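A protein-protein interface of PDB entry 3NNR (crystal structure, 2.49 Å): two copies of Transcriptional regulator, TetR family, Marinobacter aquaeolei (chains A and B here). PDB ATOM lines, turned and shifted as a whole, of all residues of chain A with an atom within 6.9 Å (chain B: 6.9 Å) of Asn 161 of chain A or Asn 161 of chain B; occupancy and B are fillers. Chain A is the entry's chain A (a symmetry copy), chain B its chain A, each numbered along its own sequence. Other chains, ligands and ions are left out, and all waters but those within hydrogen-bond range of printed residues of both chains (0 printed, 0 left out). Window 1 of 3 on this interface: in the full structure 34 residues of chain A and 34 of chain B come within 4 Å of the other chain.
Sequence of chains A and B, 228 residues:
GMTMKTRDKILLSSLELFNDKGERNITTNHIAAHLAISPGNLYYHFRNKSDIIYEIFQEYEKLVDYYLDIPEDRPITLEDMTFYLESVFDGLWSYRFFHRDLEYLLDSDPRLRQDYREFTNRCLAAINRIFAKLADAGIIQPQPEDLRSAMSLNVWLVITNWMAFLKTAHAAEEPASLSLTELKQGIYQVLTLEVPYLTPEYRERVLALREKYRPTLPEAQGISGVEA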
ATOM      1  N   LEU A  92      -7.947 -22.449  -7.879  1.00  0.00           N
ATOM      2  CA  LEU A  92      -7.355 -22.057  -6.618  1.00  0.00           C
ATOM      3  C   LEU A  92      -8.367 -21.387  -5.655  1.00  0.00           C
ATOM      4  O   LEU A  92      -8.252 -21.556  -4.435  1.00  0.00           O
ATOM      5  CB  LEU A  92      -6.137 -21.154  -6.841  1.00  0.00           C
ATOM      6  CG  LEU A  92      -4.892 -21.791  -7.485  1.00  0.00           C
ATOM      7  CD1 LEU A  92      -3.901 -20.678  -7.815  1.00  0.00           C
ATOM      8  CD2 LEU A  92      -4.234 -22.789  -6.572  1.00  0.00           C
ATOM      9  N   VAL A 155       6.436 -18.682 -12.094  1.00  0.00           N
ATOM     10  CA  VAL A 155       4.999 -18.638 -12.401  1.00  0.00           C
ATOM     11  C   VAL A 155       4.223 -19.413 -11.334  1.00  0.00           C
ATOM     12  O   VAL A 155       3.319 -18.859 -10.722  1.00  0.00           O
ATOM     13  CB  VAL A 155       4.671 -19.206 -13.786  1.00  0.00           C
ATOM     14  CG1 VAL A 155       3.204 -19.425 -13.929  1.00  0.00           C
ATOM     15  CG2 VAL A 155       5.144 -18.265 -14.836  1.00  0.00           C
ATOM     16  N   TRP A 156       4.659 -20.639 -11.050  1.00  0.00           N
ATOM     17  CA  TRP A 156       4.012 -21.482 -10.062  1.00  0.00           C
ATOM     18  C   TRP A 156       4.026 -20.806  -8.713  1.00  0.00           C
ATOM     19  O   TRP A 156       2.989 -20.744  -8.045  1.00  0.00           O
ATOM     20  CB  TRP A 156       4.690 -22.862 -10.003  1.00  0.00           C
ATOM     21  CG  TRP A 156       3.977 -23.889  -9.179  1.00  0.00           C
ATOM     22  CD1 TRP A 156       3.107 -24.856  -9.635  1.00  0.00           C
ATOM     23  CD2 TRP A 156       4.067 -24.073  -7.758  1.00  0.00           C
ATOM     24  NE1 TRP A 156       2.652 -25.611  -8.580  1.00  0.00           N
ATOM     25  CE2 TRP A 156       3.231 -25.158  -7.422  1.00  0.00           C
ATOM     26  CE3 TRP A 156       4.784 -23.426  -6.734  1.00  0.00           C
ATOM     27  CZ2 TRP A 156       3.076 -25.607  -6.106  1.00  0.00           C
ATOM     28  CZ3 TRP A 156       4.631 -23.872  -5.408  1.00  0.00           C
ATOM     29  CH2 TRP A 156       3.779 -24.949  -5.111  1.00  0.00           C
ATOM     30  N   LEU A 157       5.196 -20.306  -8.317  1.00  0.00           N
ATOM     31  CA  LEU A 157       5.388 -19.659  -7.018  1.00  0.00           C
ATOM     32  C   LEU A 157       4.459 -18.444  -6.848  1.00  0.00           C
ATOM     33  O   LEU A 157       3.879 -18.248  -5.786  1.00  0.00           O
ATOM     34  CB  LEU A 157       6.869 -19.255  -6.823  1.00  0.00           C
ATOM     35  CG  LEU A 157       7.907 -20.378  -6.609  1.00  0.00           C
ATOM     36  CD1 LEU A 157       9.361 -19.878  -6.712  1.00  0.00           C
ATOM     37  CD2 LEU A 157       7.724 -21.027  -5.243  1.00  0.00           C
ATOM     38  N   VAL A 158       4.308 -17.654  -7.907  1.00  0.00           N
ATOM     39  CA  VAL A 158       3.439 -16.475  -7.895  1.00  0.00           C
ATOM     40  C   VAL A 158       1.970 -16.853  -7.862  1.00  0.00           C
ATOM     41  O   VAL A 158       1.226 -16.297  -7.079  1.00  0.00           O
ATOM     42  CB  VAL A 158       3.712 -15.532  -9.095  1.00  0.00           C
ATOM     43  CG1 VAL A 158       2.550 -14.544  -9.316  1.00  0.00           C
ATOM     44  CG2 VAL A 158       5.050 -14.801  -8.885  1.00  0.00           C
ATOM     45  N   ILE A 159       1.561 -17.785  -8.703  1.00  0.00           N
ATOM     46  CA  ILE A 159       0.147 -18.160  -8.795  1.00  0.00           C
ATOM     47  C   ILE A 159      -0.371 -18.775  -7.504  1.00  0.00           C
ATOM     48  O   ILE A 159      -1.357 -18.327  -6.958  1.00  0.00           O
ATOM     49  CB  ILE A 159      -0.136 -19.110  -9.965  1.00  0.00           C
ATOM     50  CG1 ILE A 159       0.082 -18.387 -11.293  1.00  0.00           C
ATOM     51  CG2 ILE A 159      -1.574 -19.526  -9.952  1.00  0.00           C
ATOM     52  CD1 ILE A 159      -0.172 -19.242 -12.533  1.00  0.00           C
ATOM     53  N   THR A 160       0.346 -19.751  -6.991  1.00  0.00           N
ATOM     54  CA  THR A 160      -0.089 -20.479  -5.796  1.00  0.00           C
ATOM     55  C   THR A 160       0.031 -19.711  -4.501  1.00  0.00           C
ATOM     56  O   THR A 160      -0.509 -20.171  -3.519  1.00  0.00           O
ATOM     57  CB  THR A 160       0.633 -21.823  -5.665  1.00  0.00           C
ATOM     58  OG1 THR A 160       2.035 -21.618  -5.476  1.00  0.00           O
ATOM     59  CG2 THR A 160       0.392 -22.630  -6.896  1.00  0.00           C
ATOM     60  N   ASN A 161       0.722 -18.572  -4.484  1.00  0.00           N
ATOM     61  CA  ASN A 161       0.818 -17.727  -3.301  1.00  0.00           C
ATOM     62  C   ASN A 161      -0.014 -16.427  -3.389  1.00  0.00           C
ATOM     63  O   ASN A 161       0.104 -15.555  -2.501  1.00  0.00           O
ATOM     64  CB  ASN A 161       2.305 -17.329  -3.070  1.00  0.00           C
ATOM     65  CG  ASN A 161       2.634 -16.989  -1.591  1.00  0.00           C
ATOM     66  OD1 ASN A 161       2.094 -17.616  -0.664  1.00  0.00           O
ATOM     67  ND2 ASN A 161       3.554 -16.010  -1.374  1.00  0.00           N
ATOM     68  N   TRP A 162      -0.852 -16.275  -4.420  1.00  0.00           N
ATOM     69  CA  TRP A 162      -1.610 -15.027  -4.608  1.00  0.00           C
ATOM     70  C   TRP A 162      -2.736 -14.874  -3.581  1.00  0.00           C
ATOM     71  O   TRP A 162      -2.872 -13.796  -3.016  1.00  0.00           O
ATOM     72  CB  TRP A 162      -2.153 -14.933  -6.038  1.00  0.00           C
ATOM     73  CG  TRP A 162      -2.818 -13.616  -6.308  1.00  0.00           C
ATOM     74  CD1 TRP A 162      -4.128 -13.406  -6.588  1.00  0.00           C
ATOM     75  CD2 TRP A 162      -2.202 -12.329  -6.267  1.00  0.00           C
ATOM     76  NE1 TRP A 162      -4.369 -12.061  -6.756  1.00  0.00           N
ATOM     77  CE2 TRP A 162      -3.205 -11.378  -6.552  1.00  0.00           C
ATOM     78  CE3 TRP A 162      -0.888 -11.882  -6.018  1.00  0.00           C
ATOM     79  CZ2 TRP A 162      -2.943  -9.997  -6.603  1.00  0.00           C
ATOM     80  CZ3 TRP A 162      -0.633 -10.533  -6.048  1.00  0.00           C
ATOM     81  CH2 TRP A 162      -1.651  -9.595  -6.362  1.00  0.00           C
ATOM     82  N   MET A 163      -3.552 -15.925  -3.407  1.00  0.00           N
ATOM     83  CA  MET A 163      -4.647 -15.955  -2.421  1.00  0.00           C
ATOM     84  C   MET A 163      -4.021 -15.474  -1.077  1.00  0.00           C
ATOM     85  O   MET A 163      -4.393 -14.404  -0.531  1.00  0.00           O
ATOM     86  CB  MET A 163      -5.239 -17.399  -2.310  1.00  0.00           C
ATOM     87  CG  MET A 163      -6.781 -17.565  -2.478  1.00  0.00           C
ATOM     88  SD  MET A 163      -7.293 -17.280  -4.321  1.00  0.00           S
ATOM     89  CE  MET A 163      -7.246 -15.364  -4.337  1.00  0.00           C
ATOM     90  N   ALA A 164      -3.025 -16.232  -0.601  1.00  0.00           N
ATOM     91  CA  ALA A 164      -2.310 -15.940   0.658  1.00  0.00           C
ATOM     92  C   ALA A 164      -1.857 -14.500   0.815  1.00  0.00           C
ATOM     93  O   ALA A 164      -1.939 -13.945   1.921  1.00  0.00           O
ATOM     94  CB  ALA A 164      -1.115 -16.925   0.850  1.00  0.00           C
ATOM     95  N   PHE A 165      -1.397 -13.878  -0.270  1.00  0.00           N
ATOM     96  CA  PHE A 165      -1.019 -12.434  -0.228  1.00  0.00           C
ATOM     97  C   PHE A 165      -2.226 -11.518  -0.015  1.00  0.00           C
ATOM     98  O   PHE A 165      -2.121 -10.509   0.691  1.00  0.00           O
ATOM     99  CB  PHE A 165      -0.261 -11.977  -1.490  1.00  0.00           C
ATOM    100  CG  PHE A 165      -0.022 -10.461  -1.562  1.00  0.00           C
ATOM    101  CD1 PHE A 165       0.856  -9.838  -0.703  1.00  0.00           C
ATOM    102  CD2 PHE A 165      -0.710  -9.667  -2.482  1.00  0.00           C
ATOM    103  CE1 PHE A 165       1.084  -8.420  -0.758  1.00  0.00           C
ATOM    104  CE2 PHE A 165      -0.496  -8.260  -2.563  1.00  0.00           C
ATOM    105  CZ  PHE A 165       0.408  -7.637  -1.688  1.00  0.00           C
ATOM    106  N   LEU A 166      -3.338 -11.837  -0.680  1.00  0.00           N
ATOM    107  CA  LEU A 166      -4.570 -11.050  -0.583  1.00  0.00           C
ATOM    108  C   LEU A 166      -5.103 -11.015   0.839  1.00  0.00           C
ATOM    109  O   LEU A 166      -5.500  -9.928   1.273  1.00  0.00           O
ATOM    110  CB  LEU A 166      -5.655 -11.535  -1.567  1.00  0.00           C
ATOM    111  CG  LEU A 166      -5.371 -11.328  -3.063  1.00  0.00           C
ATOM    112  CD1 LEU A 166      -6.380 -12.073  -3.876  1.00  0.00           C
ATOM    113  CD2 LEU A 166      -5.356  -9.877  -3.447  1.00  0.00           C
ATOM    114  N   LEU B  92      13.010 -16.408   7.513  1.00  0.00           N
ATOM    115  CA  LEU B  92      11.915 -17.269   7.121  1.00  0.00           C
ATOM    116  C   LEU B  92      12.082 -18.727   7.618  1.00  0.00           C
ATOM    117  O   LEU B  92      11.082 -19.384   7.929  1.00  0.00           O
ATOM    118  CB  LEU B  92      11.705 -17.233   5.603  1.00  0.00           C
ATOM    119  CG  LEU B  92      11.187 -15.918   4.993  1.00  0.00           C
ATOM    120  CD1 LEU B  92      11.267 -16.032   3.472  1.00  0.00           C
ATOM    121  CD2 LEU B  92       9.766 -15.631   5.396  1.00  0.00           C
ATOM    122  N   VAL B 155       9.001 -10.501  -6.193  1.00  0.00           N
ATOM    123  CA  VAL B 155      10.081 -10.878  -5.269  1.00  0.00           C
ATOM    124  C   VAL B 155       9.480 -11.387  -3.958  1.00  0.00           C
ATOM    125  O   VAL B 155       9.789 -12.496  -3.542  1.00  0.00           O
ATOM    126  CB  VAL B 155      11.042  -9.721  -4.978  1.00  0.00           C
ATOM    127  CG1 VAL B 155      11.923 -10.048  -3.821  1.00  0.00           C
ATOM    128  CG2 VAL B 155      11.873  -9.445  -6.180  1.00  0.00           C
ATOM    129  N   TRP B 156       8.551 -10.621  -3.390  1.00  0.00           N
ATOM    130  CA  TRP B 156       7.905 -10.984  -2.143  1.00  0.00           C
ATOM    131  C   TRP B 156       7.196 -12.309  -2.291  1.00  0.00           C
ATOM    132  O   TRP B 156       7.354 -13.190  -1.441  1.00  0.00           O
ATOM    133  CB  TRP B 156       6.933  -9.878  -1.695  1.00  0.00           C
ATOM    134  CG  TRP B 156       6.372 -10.040  -0.317  1.00  0.00           C
ATOM    135  CD1 TRP B 156       6.836  -9.451   0.839  1.00  0.00           C
ATOM    136  CD2 TRP B 156       5.236 -10.830   0.067  1.00  0.00           C
ATOM    137  NE1 TRP B 156       6.063  -9.842   1.907  1.00  0.00           N
ATOM    138  CE2 TRP B 156       5.072 -10.678   1.460  1.00  0.00           C
ATOM    139  CE3 TRP B 156       4.335 -11.649  -0.637  1.00  0.00           C
ATOM    140  CZ2 TRP B 156       4.054 -11.323   2.170  1.00  0.00           C
ATOM    141  CZ3 TRP B 156       3.310 -12.302   0.073  1.00  0.00           C
ATOM    142  CH2 TRP B 156       3.185 -12.136   1.462  1.00  0.00           C
ATOM    143  N   LEU B 157       6.418 -12.443  -3.365  1.00  0.00           N
ATOM    144  CA  LEU B 157       5.629 -13.646  -3.633  1.00  0.00           C
ATOM    145  C   LEU B 157       6.521 -14.896  -3.739  1.00  0.00           C
ATOM    146  O   LEU B 157       6.182 -15.949  -3.212  1.00  0.00           O
ATOM    147  CB  LEU B 157       4.774 -13.466  -4.910  1.00  0.00           C
ATOM    148  CG  LEU B 157       3.581 -12.489  -4.855  1.00  0.00           C
ATOM    149  CD1 LEU B 157       2.991 -12.183  -6.245  1.00  0.00           C
ATOM    150  CD2 LEU B 157       2.467 -13.049  -3.980  1.00  0.00           C
ATOM    151  N   VAL B 158       7.668 -14.758  -4.399  1.00  0.00           N
ATOM    152  CA  VAL B 158       8.623 -15.857  -4.560  1.00  0.00           C
ATOM    153  C   VAL B 158       9.318 -16.199  -3.256  1.00  0.00           C
ATOM    154  O   VAL B 158       9.411 -17.362  -2.916  1.00  0.00           O
ATOM    155  CB  VAL B 158       9.679 -15.560  -5.656  1.00  0.00           C
ATOM    156  CG1 VAL B 158      10.899 -16.494  -5.536  1.00  0.00           C
ATOM    157  CG2 VAL B 158       9.024 -15.654  -7.046  1.00  0.00           C
ATOM    158  N   ILE B 159       9.799 -15.201  -2.539  1.00  0.00           N
ATOM    159  CA  ILE B 159      10.552 -15.442  -1.305  1.00  0.00           C
ATOM    160  C   ILE B 159       9.701 -16.103  -0.232  1.00  0.00           C
ATOM    161  O   ILE B 159      10.063 -17.132   0.298  1.00  0.00           O
ATOM    162  CB  ILE B 159      11.186 -14.165  -0.742  1.00  0.00           C
ATOM    163  CG1 ILE B 159      12.281 -13.664  -1.682  1.00  0.00           C
ATOM    164  CG2 ILE B 159      11.862 -14.460   0.561  1.00  0.00           C
ATOM    165  CD1 ILE B 159      12.984 -12.390  -1.219  1.00  0.00           C
ATOM    166  N   THR B 160       8.539 -15.542   0.023  1.00  0.00           N
ATOM    167  CA  THR B 160       7.665 -16.035   1.091  1.00  0.00           C
ATOM    168  C   THR B 160       6.967 -17.342   0.793  1.00  0.00           C
ATOM    169  O   THR B 160       6.409 -17.906   1.709  1.00  0.00           O
ATOM    170  CB  THR B 160       6.630 -14.983   1.499  1.00  0.00           C
ATOM    171  OG1 THR B 160       5.750 -14.701   0.409  1.00  0.00           O
ATOM    172  CG2 THR B 160       7.339 -13.740   1.923  1.00  0.00           C
ATOM    173  N   ASN B 161       6.986 -17.818  -0.451  1.00  0.00           N
ATOM    174  CA  ASN B 161       6.413 -19.109  -0.808  1.00  0.00           C
ATOM    175  C   ASN B 161       7.464 -20.205  -1.100  1.00  0.00           C
ATOM    176  O   ASN B 161       7.097 -21.308  -1.558  1.00  0.00           O
ATOM    177  CB  ASN B 161       5.527 -18.946  -2.078  1.00  0.00           C
ATOM    178  CG  ASN B 161       4.411 -20.020  -2.198  1.00  0.00           C
ATOM    179  OD1 ASN B 161       3.828 -20.441  -1.186  1.00  0.00           O
ATOM    180  ND2 ASN B 161       4.092 -20.439  -3.454  1.00  0.00           N
ATOM    181  N   TRP B 162       8.749 -19.939  -0.841  1.00  0.00           N
ATOM    182  CA  TRP B 162       9.808 -20.907  -1.173  1.00  0.00           C
ATOM    183  C   TRP B 162       9.797 -22.120  -0.237  1.00  0.00           C
ATOM    184  O   TRP B 162       9.890 -23.239  -0.726  1.00  0.00           O
ATOM    185  CB  TRP B 162      11.181 -20.227  -1.177  1.00  0.00           C
ATOM    186  CG  TRP B 162      12.270 -21.148  -1.640  1.00  0.00           C
ATOM    187  CD1 TRP B 162      13.321 -21.600  -0.911  1.00  0.00           C
ATOM    188  CD2 TRP B 162      12.374 -21.765  -2.923  1.00  0.00           C
ATOM    189  NE1 TRP B 162      14.098 -22.445  -1.671  1.00  0.00           N
ATOM    190  CE2 TRP B 162      13.531 -22.571  -2.906  1.00  0.00           C
ATOM    191  CE3 TRP B 162      11.595 -21.712  -4.098  1.00  0.00           C
ATOM    192  CZ2 TRP B 162      13.945 -23.323  -4.021  1.00  0.00           C
ATOM    193  CZ3 TRP B 162      11.985 -22.460  -5.182  1.00  0.00           C
ATOM    194  CH2 TRP B 162      13.168 -23.245  -5.152  1.00  0.00           C
ATOM    195  N   MET B 163       9.750 -21.874   1.082  1.00  0.00           N
ATOM    196  CA  MET B 163       9.680 -22.930   2.107  1.00  0.00           C
ATOM    197  C   MET B 163       8.541 -23.890   1.651  1.00  0.00           C
ATOM    198  O   MET B 163       8.781 -25.082   1.331  1.00  0.00           O
ATOM    199  CB  MET B 163       9.394 -22.305   3.512  1.00  0.00           C
ATOM    200  CG  MET B 163      10.357 -22.679   4.682  1.00  0.00           C
ATOM    201  SD  MET B 163      12.079 -21.835   4.434  1.00  0.00           S
ATOM    202  CE  MET B 163      12.800 -23.036   3.125  1.00  0.00           C
ATOM    203  N   ALA B 164       7.325 -23.337   1.555  1.00  0.00           N
ATOM    204  CA  ALA B 164       6.120 -24.085   1.141  1.00  0.00           C
ATOM    205  C   ALA B 164       6.296 -24.940  -0.101  1.00  0.00           C
ATOM    206  O   ALA B 164       5.770 -26.062  -0.158  1.00  0.00           O
ATOM    207  CB  ALA B 164       4.902 -23.122   0.988  1.00  0.00           C
ATOM    208  N   PHE B 165       7.036 -24.442  -1.091  1.00  0.00           N
ATOM    209  CA  PHE B 165       7.339 -25.251  -2.309  1.00  0.00           C
ATOM    210  C   PHE B 165       8.249 -26.445  -2.009  1.00  0.00           C
ATOM    211  O   PHE B 165       8.073 -27.520  -2.591  1.00  0.00           O
ATOM    212  CB  PHE B 165       7.967 -24.416  -3.441  1.00  0.00           C
ATOM    213  CG  PHE B 165       8.461 -25.249  -4.634  1.00  0.00           C
ATOM    214  CD1 PHE B 165       7.572 -25.881  -5.476  1.00  0.00           C
ATOM    215  CD2 PHE B 165       9.826 -25.412  -4.883  1.00  0.00           C
ATOM    216  CE1 PHE B 165       8.022 -26.668  -6.591  1.00  0.00           C
ATOM    217  CE2 PHE B 165      10.297 -26.179  -5.988  1.00  0.00           C
ATOM    218  CZ  PHE B 165       9.383 -26.812  -6.844  1.00  0.00           C
ATOM    219  N   LEU B 166       9.254 -26.225  -1.158  1.00  0.00           N
ATOM    220  CA  LEU B 166      10.212 -27.268  -0.782  1.00  0.00           C
ATOM    221  C   LEU B 166       9.526 -28.439  -0.099  1.00  0.00           C
ATOM    222  O   LEU B 166       9.868 -29.578  -0.438  1.00  0.00           O
ATOM    223  CB  LEU B 166      11.363 -26.721   0.087  1.00  0.00           C
ATOM    224  CG  LEU B 166      12.341 -25.751  -0.596  1.00  0.00           C
ATOM    225  CD1 LEU B 166      13.227 -25.122   0.430  1.00  0.00           C
ATOM    226  CD2 LEU B 166      13.163 -26.422  -1.658  1.00  0.00           C
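O of Trp 156 of chain B sits at hydrogen-bond distance from OG1 of Thr 160 of chain B, 2.9 Å away.
O of Trp 156 of chain A is in hydrogen-bond range of OG1 of Thr 160 of chain A, 2.9 Å away.
OG1 of Thr 160 of chain B is in hydrogen-bond range of ND2 of Asn 161 of chain A (3.1 Å).
ND2 of Asn 161 of chain B sits at hydrogen-bond distance from OG1 of Thr 160 of chain A, at 3.1 Å.
ND2 of Asn 161 of chain B sits at hydrogen-bond distance from O of Leu 157 of chain A, 3.2 Å away.
O of Leu 157 of chain B is in hydrogen-bond range of ND2 of Asn 161 of chain A.
The side-chain amide oxygen (OD1) of Asn 161 of chain B sits close to the side-chain amide oxygen (OD1) of Asn 161 of chain A (3.4 Å).
Hydrophobic or aromatic side chains of chain A that line the printed part of chain B: Trp 156, Leu 157, Val 158, Trp 162 and Phe 165.
Hydrophobic or aromatic side chains of chain B that line the printed part of chain A: Trp 156, Leu 157, Val 158, Trp 162 and Phe 165.
Among the printed residues, no Asp or Glu carboxylate lies within 4 Å of a Lys or Arg side-chain nitrogen of the other chain.
Printed residues of chain B within 4 Å of Asn 161 of chain A: Trp 156, Leu 157, Thr 160 and Asn 161.
Of the printed residues of chain B, Val 158 of chain A touches Leu 157.
Printed residues of chain B within 4 Å of Thr 160 of chain A: Asn 161 (3.1 Å).
The nearest printed residue of chain A that does not touch Asn 161 of chain B is Val 158 of chain A (5.3 Å).
Trp 156 of chain A touches Asn 161 of chain B.
Trp 156 of chain A touches Phe 165 of chain B.
Leu 157 of chain A touches Val 158 of chain B (CD1 to CG1, 3.9 Å).
Leu 157 of chain A touches Trp 162 of chain B.
Phe 165 of chain B touches Leu 157 of chain A.
Leu 157 of chain B touches Val 158 of chain A (CD1 to CG1, 3.9 Å).
Asn 161 of chain A touches Trp 156 of chain B.
CD1 of Leu 157 of chain B touches CE3 of Trp 162 of chain A, 3.9 Å away.
CD1 of Phe 165 of chain A touches CZ3 of Trp 156 of chain B, at 3.6 Å.
Leu 157 of chain B touches Phe 165 of chain A (CD2 to CB, 3.8 Å).
Trp 156 of chain A touches Asn 161 of chain B, and with the chains exchanged Asn 161 of chain A touches Trp 156 of chain B.
Leu 157 of chain A touches Val 158 of chain B, and with the chains exchanged Val 158 of chain A touches Leu 157 of chain B.
Leu 157 of chain A touches Trp 162 of chain B, and with the chains exchanged Trp 162 of chain A touches Leu 157 of chain B.
Asn 161 of chain A touches its own counterpart, Asn 161 of chain B.
Of the 15 pairs that touch across the chains among the printed residues, 15 have their exchanged pair printed and touching as well.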
